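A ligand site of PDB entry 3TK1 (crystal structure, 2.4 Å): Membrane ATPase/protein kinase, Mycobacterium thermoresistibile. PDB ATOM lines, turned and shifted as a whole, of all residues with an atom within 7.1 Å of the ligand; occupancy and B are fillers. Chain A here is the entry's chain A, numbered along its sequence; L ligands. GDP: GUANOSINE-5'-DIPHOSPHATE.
The backbone NH (N) of Gly 66 is in hydrogen-bond range of an oxygen (O3B) of the ligand (3.0 Å). An oxygen (O2B) of the ligand sits at hydrogen-bond distance from the backbone NH of Lys 69. The backbone NH (N) of Gly 68 sits at hydrogen-bond distance from an oxygen (O3A) of the ligand, at 3.1 Å. O1B of the ligand lies within hydrogen-bond range of N of Ser 70 (2.9 Å). The side-chain hydroxyl (OG1) of Thr 71 lies within hydrogen-bond range of an oxygen (O1A) of the ligand (2.8 Å). An oxygen (O6) of the ligand lies close to the side-chain amide oxygen (OD1) of Asn 202, 3.2 Å away. The side-chain amino group of Lys 203 sits at hydrogen-bond distance from an oxygen (O4') of the ligand, 3.4 Å away. N of Ala 242 lies within hydrogen-bond range of O6 of the ligand, 3.0 Å away. The backbone NH of Leu 243 sits at hydrogen-bond distance from an oxygen (O6) of the ligand (3.2 Å). The side-chain carboxylate (OD2) of Asp 205 sits at hydrogen-bond distance from a nitrogen (N1) of the ligand, 2.7 Å away.
O of Val 67 is in hydrogen-bond range of ND2 of Asn 202 (3.3 Å). N of Ala 242 sits at hydrogen-bond distance from OD1 of Asn 202, at 3.0 Å. The side-chain hydroxyl (OG) of Ser 241 lies within hydrogen-bond range of the backbone NH (N) of Glu 244, at 3.2 Å. The backbone carbonyl oxygen of Met 240 sits at hydrogen-bond distance from the backbone NH of Lys 203 (3.0 Å). NZ of Lys 203 lies within hydrogen-bond range of O of Gly 66 (2.9 Å). The backbone carbonyl oxygen (O) of Gly 68 is in hydrogen-bond range of the side-chain hydroxyl (OG) of Ser 72 (2.7 Å). The side-chain carboxylate (OE2) of Glu 155 is in salt-bridge range of the side-chain amino group (NZ) of Lys 69, 2.5 Å away. The backbone carbonyl oxygen (O) of Lys 203 is in hydrogen-bond range of a ring nitrogen (ND1) of His 208, at 3.2 Å.
Merely in contact with the ligand: Ser 241 (3.6 Å), Pro 65 (3.6 Å), Val 67 (3.7 Å) and Val 64 (3.8 Å). Hydrophobic or aromatic side chains that line the ligand: Val 67, Ala 242 and Leu 243. Of the 26 residues printed, 14 come within 4 Å of the ligand. Along chain A the residues within 4 Å of the ligand span positions 64 to 243.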
ATOM      1  N   GLY A  63     -10.037 -12.029  24.155  1.00  0.00           N
ATOM      2  CA  GLY A  63     -11.205 -12.849  23.803  1.00  0.00           C
ATOM      3  C   GLY A  63     -12.162 -12.868  24.967  1.00  0.00           C
ATOM      4  O   GLY A  63     -11.743 -12.709  26.114  1.00  0.00           O
ATOM      5  N   VAL A  64     -13.444 -13.044  24.709  1.00  0.00           N
ATOM      6  CA  VAL A  64     -14.416 -13.018  25.805  1.00  0.00           C
ATOM      7  C   VAL A  64     -14.231 -14.245  26.699  1.00  0.00           C
ATOM      8  O   VAL A  64     -13.836 -15.303  26.218  1.00  0.00           O
ATOM      9  CB  VAL A  64     -15.866 -12.952  25.318  1.00  0.00           C
ATOM     10  CG1 VAL A  64     -16.030 -11.900  24.222  1.00  0.00           C
ATOM     11  CG2 VAL A  64     -16.326 -14.310  24.850  1.00  0.00           C
ATOM     12  N   PRO A  65     -14.505 -14.095  28.002  1.00  0.00           N
ATOM     13  CA  PRO A  65     -14.499 -15.236  28.923  1.00  0.00           C
ATOM     14  C   PRO A  65     -15.219 -16.461  28.353  1.00  0.00           C
ATOM     15  O   PRO A  65     -16.302 -16.327  27.780  1.00  0.00           O
ATOM     16  CB  PRO A  65     -15.238 -14.692  30.135  1.00  0.00           C
ATOM     17  CG  PRO A  65     -14.904 -13.236  30.156  1.00  0.00           C
ATOM     18  CD  PRO A  65     -14.724 -12.822  28.701  1.00  0.00           C
ATOM     19  N   GLY A  66     -14.596 -17.635  28.496  1.00  0.00           N
ATOM     20  CA  GLY A  66     -15.157 -18.873  27.976  1.00  0.00           C
ATOM     21  C   GLY A  66     -14.641 -19.249  26.602  1.00  0.00           C
ATOM     22  O   GLY A  66     -14.850 -20.397  26.162  1.00  0.00           O
ATOM     23  N   VAL A  67     -13.932 -18.324  25.930  1.00  0.00           N
ATOM     24  CA  VAL A  67     -13.433 -18.569  24.573  1.00  0.00           C
ATOM     25  C   VAL A  67     -12.257 -19.561  24.532  1.00  0.00           C
ATOM     26  O   VAL A  67     -12.002 -20.175  23.495  1.00  0.00           O
ATOM     27  CB  VAL A  67     -13.052 -17.248  23.838  1.00  0.00           C
ATOM     28  CG1 VAL A  67     -11.763 -16.679  24.420  1.00  0.00           C
ATOM     29  CG2 VAL A  67     -12.884 -17.484  22.335  1.00  0.00           C
ATOM     30  N   GLY A  68     -11.560 -19.750  25.662  1.00  0.00           N
ATOM     31  CA  GLY A  68     -10.393 -20.658  25.736  1.00  0.00           C
ATOM     32  C   GLY A  68      -9.045 -19.969  25.926  1.00  0.00           C
ATOM     33  O   GLY A  68      -7.988 -20.536  25.615  1.00  0.00           O
ATOM     34  N   LYS A  69      -9.081 -18.766  26.464  1.00  0.00           N
ATOM     35  CA  LYS A  69      -7.890 -17.950  26.587  1.00  0.00           C
ATOM     36  C   LYS A  69      -6.814 -18.575  27.499  1.00  0.00           C
ATOM     37  O   LYS A  69      -5.626 -18.592  27.144  1.00  0.00           O
ATOM     38  CB  LYS A  69      -8.292 -16.571  27.057  1.00  0.00           C
ATOM     39  CG  LYS A  69      -7.241 -15.524  26.896  1.00  0.00           C
ATOM     40  CD  LYS A  69      -7.833 -14.121  26.804  1.00  0.00           C
ATOM     41  CE  LYS A  69      -8.685 -13.761  28.012  1.00  0.00           C
ATOM     42  NZ  LYS A  69      -7.997 -13.897  29.338  1.00  0.00           N
ATOM     43  N   SER A  70      -7.225 -19.093  28.657  1.00  0.00           N
ATOM     44  CA  SER A  70      -6.235 -19.631  29.617  1.00  0.00           C
ATOM     45  C   SER A  70      -5.610 -20.891  29.055  1.00  0.00           C
ATOM     46  O   SER A  70      -4.407 -21.066  29.107  1.00  0.00           O
ATOM     47  CB  SER A  70      -6.840 -19.931  31.016  1.00  0.00           C
ATOM     48  OG  SER A  70      -6.345 -19.050  32.018  1.00  0.00           O
ATOM     49  N   THR A  71      -6.448 -21.765  28.518  1.00  0.00           N
ATOM     50  CA  THR A  71      -5.956 -22.975  27.899  1.00  0.00           C
ATOM     51  C   THR A  71      -5.010 -22.653  26.747  1.00  0.00           C
ATOM     52  O   THR A  71      -4.027 -23.356  26.534  1.00  0.00           O
ATOM     53  CB  THR A  71      -7.124 -23.827  27.379  1.00  0.00           C
ATOM     54  OG1 THR A  71      -8.142 -23.919  28.379  1.00  0.00           O
ATOM     55  CG2 THR A  71      -6.634 -25.236  26.976  1.00  0.00           C
ATOM     56  N   SER A  72      -5.317 -21.596  26.005  1.00  0.00           N
ATOM     57  CA  SER A  72      -4.509 -21.209  24.851  1.00  0.00           C
ATOM     58  C   SER A  72      -3.129 -20.725  25.282  1.00  0.00           C
ATOM     59  O   SER A  72      -2.111 -21.121  24.715  1.00  0.00           O
ATOM     60  CB  SER A  72      -5.222 -20.095  24.053  1.00  0.00           C
ATOM     61  OG  SER A  72      -6.409 -20.572  23.448  1.00  0.00           O
ATOM     62  N   ARG A 112       3.194 -16.380  35.733  1.00  0.00           N
ATOM     63  CA  ARG A 112       1.838 -15.884  35.535  1.00  0.00           C
ATOM     64  C   ARG A 112       1.530 -14.798  36.555  1.00  0.00           C
ATOM     65  O   ARG A 112       1.425 -15.075  37.737  1.00  0.00           O
ATOM     66  CB  ARG A 112       0.827 -17.025  35.598  1.00  0.00           C
ATOM     67  CG  ARG A 112      -0.493 -16.631  34.988  1.00  0.00           C
ATOM     68  CD  ARG A 112      -1.276 -17.775  34.362  1.00  0.00           C
ATOM     69  NE  ARG A 112      -2.240 -17.224  33.395  1.00  0.00           N
ATOM     70  CZ  ARG A 112      -2.918 -17.926  32.478  1.00  0.00           C
ATOM     71  NH1 ARG A 112      -2.759 -19.242  32.348  1.00  0.00           N
ATOM     72  NH2 ARG A 112      -3.757 -17.282  31.676  1.00  0.00           N
ATOM     73  N   GLU A 155      -2.585 -10.220  28.455  1.00  0.00           N
ATOM     74  CA  GLU A 155      -3.901 -10.821  28.348  1.00  0.00           C
ATOM     75  C   GLU A 155      -4.907  -9.838  28.927  1.00  0.00           C
ATOM     76  O   GLU A 155      -4.626  -9.201  29.941  1.00  0.00           O
ATOM     77  CB  GLU A 155      -3.863 -12.123  29.164  1.00  0.00           C
ATOM     78  CG  GLU A 155      -5.190 -12.761  29.515  1.00  0.00           C
ATOM     79  CD  GLU A 155      -5.072 -14.040  30.344  1.00  0.00           C
ATOM     80  OE1 GLU A 155      -4.212 -14.129  31.223  1.00  0.00           O
ATOM     81  OE2 GLU A 155      -5.906 -14.942  30.143  1.00  0.00           O
ATOM     82  N   LEU A 176      -9.077 -14.108  20.011  1.00  0.00           N
ATOM     83  CA  LEU A 176      -9.704 -15.430  20.001  1.00  0.00           C
ATOM     84  C   LEU A 176     -11.215 -15.323  19.936  1.00  0.00           C
ATOM     85  O   LEU A 176     -11.835 -14.521  20.639  1.00  0.00           O
ATOM     86  CB  LEU A 176      -9.325 -16.220  21.236  1.00  0.00           C
ATOM     87  CG  LEU A 176      -7.840 -16.299  21.579  1.00  0.00           C
ATOM     88  CD1 LEU A 176      -7.619 -17.172  22.807  1.00  0.00           C
ATOM     89  CD2 LEU A 176      -6.996 -16.799  20.419  1.00  0.00           C
ATOM     90  N   LEU A 178     -14.988 -17.803  18.847  1.00  0.00           N
ATOM     91  CA  LEU A 178     -15.634 -19.107  18.748  1.00  0.00           C
ATOM     92  C   LEU A 178     -16.655 -19.129  17.609  1.00  0.00           C
ATOM     93  O   LEU A 178     -17.314 -18.097  17.305  1.00  0.00           O
ATOM     94  CB  LEU A 178     -16.354 -19.432  20.063  1.00  0.00           C
ATOM     95  CG  LEU A 178     -15.536 -19.703  21.325  1.00  0.00           C
ATOM     96  CD1 LEU A 178     -16.416 -20.446  22.322  1.00  0.00           C
ATOM     97  CD2 LEU A 178     -14.246 -20.490  21.053  1.00  0.00           C
ATOM     98  N   ASN A 202     -11.069 -20.770  18.103  1.00  0.00           N
ATOM     99  CA  ASN A 202     -10.550 -21.824  18.974  1.00  0.00           C
ATOM    100  C   ASN A 202     -11.622 -22.906  19.165  1.00  0.00           C
ATOM    101  O   ASN A 202     -12.769 -22.724  18.739  1.00  0.00           O
ATOM    102  CB  ASN A 202     -10.074 -21.230  20.312  1.00  0.00           C
ATOM    103  CG  ASN A 202      -9.364 -22.232  21.194  1.00  0.00           C
ATOM    104  OD1 ASN A 202      -8.609 -23.105  20.734  1.00  0.00           O
ATOM    105  ND2 ASN A 202      -9.586 -22.113  22.493  1.00  0.00           N
ATOM    106  N   LYS A 203     -11.244 -24.026  19.777  1.00  0.00           N
ATOM    107  CA  LYS A 203     -12.157 -25.170  20.022  1.00  0.00           C
ATOM    108  C   LYS A 203     -12.494 -25.903  18.742  1.00  0.00           C
ATOM    109  O   LYS A 203     -13.527 -26.544  18.647  1.00  0.00           O
ATOM    110  CB  LYS A 203     -13.468 -24.766  20.723  1.00  0.00           C
ATOM    111  CG  LYS A 203     -13.241 -24.015  22.016  1.00  0.00           C
ATOM    112  CD  LYS A 203     -14.442 -24.061  22.932  1.00  0.00           C
ATOM    113  CE  LYS A 203     -14.209 -23.226  24.185  1.00  0.00           C
ATOM    114  NZ  LYS A 203     -15.429 -23.064  25.049  1.00  0.00           N
ATOM    115  N   ALA A 204     -11.606 -25.785  17.759  1.00  0.00           N
ATOM    116  CA  ALA A 204     -11.732 -26.530  16.518  1.00  0.00           C
ATOM    117  C   ALA A 204     -11.228 -27.937  16.798  1.00  0.00           C
ATOM    118  O   ALA A 204     -10.093 -28.293  16.478  1.00  0.00           O
ATOM    119  CB  ALA A 204     -10.919 -25.866  15.398  1.00  0.00           C
ATOM    120  N   ASP A 205     -12.094 -28.727  17.434  1.00  0.00           N
ATOM    121  CA  ASP A 205     -11.846 -30.120  17.730  1.00  0.00           C
ATOM    122  C   ASP A 205     -13.183 -30.891  17.731  1.00  0.00           C
ATOM    123  O   ASP A 205     -14.253 -30.296  17.846  1.00  0.00           O
ATOM    124  CB  ASP A 205     -11.069 -30.282  19.058  1.00  0.00           C
ATOM    125  CG  ASP A 205     -11.594 -29.350  20.161  1.00  0.00           C
ATOM    126  OD1 ASP A 205     -12.816 -29.320  20.412  1.00  0.00           O
ATOM    127  OD2 ASP A 205     -10.779 -28.650  20.798  1.00  0.00           O
ATOM    128  N   GLY A 206     -13.092 -32.204  17.579  1.00  0.00           N
ATOM    129  CA  GLY A 206     -14.260 -33.071  17.587  1.00  0.00           C
ATOM    130  C   GLY A 206     -15.119 -32.836  16.364  1.00  0.00           C
ATOM    131  O   GLY A 206     -14.611 -32.514  15.291  1.00  0.00           O
ATOM    132  N   HIS A 208     -16.980 -30.386  16.100  1.00  0.00           N
ATOM    133  CA  HIS A 208     -17.021 -28.939  15.967  1.00  0.00           C
ATOM    134  C   HIS A 208     -15.985 -28.431  14.990  1.00  0.00           C
ATOM    135  O   HIS A 208     -16.127 -27.332  14.449  1.00  0.00           O
ATOM    136  CB  HIS A 208     -16.839 -28.303  17.346  1.00  0.00           C
ATOM    137  CG  HIS A 208     -17.318 -26.871  17.448  1.00  0.00           C
ATOM    138  ND1 HIS A 208     -16.519 -25.861  17.874  1.00  0.00           N
ATOM    139  CD2 HIS A 208     -18.557 -26.305  17.184  1.00  0.00           C
ATOM    140  CE1 HIS A 208     -17.213 -24.705  17.871  1.00  0.00           C
ATOM    141  NE2 HIS A 208     -18.456 -24.976  17.442  1.00  0.00           N
ATOM    142  N   MET A 240      -7.761 -23.391  15.669  1.00  0.00           N
ATOM    143  CA  MET A 240      -6.900 -23.911  16.724  1.00  0.00           C
ATOM    144  C   MET A 240      -7.732 -24.705  17.742  1.00  0.00           C
ATOM    145  O   MET A 240      -8.914 -24.428  17.931  1.00  0.00           O
ATOM    146  CB  MET A 240      -6.232 -22.737  17.432  1.00  0.00           C
ATOM    147  CG  MET A 240      -5.230 -23.112  18.502  1.00  0.00           C
ATOM    148  SD  MET A 240      -4.344 -21.685  19.141  1.00  0.00           S
ATOM    149  CE  MET A 240      -5.483 -21.090  20.398  1.00  0.00           C
ATOM    150  N   SER A 241      -7.130 -25.737  18.342  1.00  0.00           N
ATOM    151  CA  SER A 241      -7.693 -26.385  19.519  1.00  0.00           C
ATOM    152  C   SER A 241      -6.631 -26.302  20.618  1.00  0.00           C
ATOM    153  O   SER A 241      -5.671 -27.080  20.643  1.00  0.00           O
ATOM    154  CB  SER A 241      -8.080 -27.852  19.230  1.00  0.00           C
ATOM    155  OG  SER A 241      -8.348 -28.584  20.414  1.00  0.00           O
ATOM    156  N   ALA A 242      -6.812 -25.331  21.513  1.00  0.00           N
ATOM    157  CA  ALA A 242      -5.898 -25.170  22.643  1.00  0.00           C
ATOM    158  C   ALA A 242      -5.879 -26.401  23.549  1.00  0.00           C
ATOM    159  O   ALA A 242      -4.852 -26.735  24.102  1.00  0.00           O
ATOM    160  CB  ALA A 242      -6.233 -23.927  23.447  1.00  0.00           C
ATOM    161  N   LEU A 243      -7.024 -27.067  23.690  1.00  0.00           N
ATOM    162  CA  LEU A 243      -7.121 -28.247  24.566  1.00  0.00           C
ATOM    163  C   LEU A 243      -6.315 -29.416  23.997  1.00  0.00           C
ATOM    164  O   LEU A 243      -5.694 -30.163  24.756  1.00  0.00           O
ATOM    165  CB  LEU A 243      -8.597 -28.662  24.778  1.00  0.00           C
ATOM    166  CG  LEU A 243      -9.131 -29.360  26.056  1.00  0.00           C
ATOM    167  CD1 LEU A 243      -8.248 -30.534  26.470  1.00  0.00           C
ATOM    168  CD2 LEU A 243      -9.364 -28.429  27.246  1.00  0.00           C
ATOM    169  N   GLU A 244      -6.284 -29.584  22.673  1.00  0.00           N
ATOM    170  CA  GLU A 244      -5.672 -30.763  22.095  1.00  0.00           C
ATOM    171  C   GLU A 244      -4.340 -30.485  21.346  1.00  0.00           C
ATOM    172  O   GLU A 244      -3.696 -31.417  20.845  1.00  0.00           O
ATOM    173  CB  GLU A 244      -6.730 -31.484  21.255  1.00  0.00           C
ATOM    174  CG  GLU A 244      -6.325 -32.015  19.882  1.00  0.00           C
ATOM    175  CD  GLU A 244      -7.535 -32.528  19.110  1.00  0.00           C
ATOM    176  OE1 GLU A 244      -8.521 -32.964  19.765  1.00  0.00           O
ATOM    177  OE2 GLU A 244      -7.490 -32.486  17.857  1.00  0.00           O
ATOM    178  N   GLY A 245      -3.935 -29.226  21.315  1.00  0.00           N
ATOM    179  CA  GLY A 245      -2.632 -28.838  20.762  1.00  0.00           C
ATOM    180  C   GLY A 245      -2.594 -28.488  19.282  1.00  0.00           C
ATOM    181  O   GLY A 245      -1.619 -27.922  18.804  1.00  0.00           O
HETATM  182  PB  GDP L   1     -11.104 -18.155  29.267  1.00  0.00           P
HETATM  183  O1B GDP L   1      -9.753 -18.320  29.928  1.00  0.00           O
HETATM  184  O2B GDP L   1     -11.084 -17.300  28.008  1.00  0.00           O
HETATM  185  O3B GDP L   1     -12.146 -17.677  30.241  1.00  0.00           O
HETATM  186  O3A GDP L   1     -11.515 -19.626  28.732  1.00  0.00           O
HETATM  187  PA  GDP L   1     -10.966 -21.001  29.431  1.00  0.00           P
HETATM  188  O1A GDP L   1     -10.181 -21.967  28.567  1.00  0.00           O
HETATM  189  O2A GDP L   1     -10.408 -20.604  30.774  1.00  0.00           O
HETATM  190  O5' GDP L   1     -12.328 -21.810  29.687  1.00  0.00           O
HETATM  191  C5' GDP L   1     -13.080 -22.321  28.580  1.00  0.00           C
HETATM  192  C4' GDP L   1     -13.681 -23.674  28.910  1.00  0.00           C
HETATM  193  O4' GDP L   1     -13.758 -24.412  27.681  1.00  0.00           O
HETATM  194  C3' GDP L   1     -12.855 -24.485  29.915  1.00  0.00           C
HETATM  195  O3' GDP L   1     -13.696 -24.971  31.006  1.00  0.00           O
HETATM  196  C2' GDP L   1     -12.172 -25.564  29.063  1.00  0.00           C
HETATM  197  O2' GDP L   1     -12.244 -26.876  29.659  1.00  0.00           O
HETATM  198  C1' GDP L   1     -12.845 -25.518  27.671  1.00  0.00           C
HETATM  199  N9  GDP L   1     -11.893 -25.345  26.543  1.00  0.00           N
HETATM  200  C8  GDP L   1     -10.856 -24.470  26.525  1.00  0.00           C
HETATM  201  N7  GDP L   1     -10.174 -24.519  25.344  1.00  0.00           N
HETATM  202  C5  GDP L   1     -10.765 -25.441  24.580  1.00  0.00           C
HETATM  203  C6  GDP L   1     -10.533 -25.976  23.235  1.00  0.00           C
HETATM  204  O6  GDP L   1      -9.579 -25.572  22.539  1.00  0.00           O
HETATM  205  N1  GDP L   1     -11.356 -26.931  22.788  1.00  0.00           N
HETATM  206  C2  GDP L   1     -12.384 -27.396  23.527  1.00  0.00           C
HETATM  207  N2  GDP L   1     -13.180 -28.355  22.996  1.00  0.00           N
HETATM  208  N3  GDP L   1     -12.669 -26.946  24.783  1.00  0.00           N
HETATM  209  C4  GDP L   1     -11.896 -25.984  25.360  1.00  0.00           C
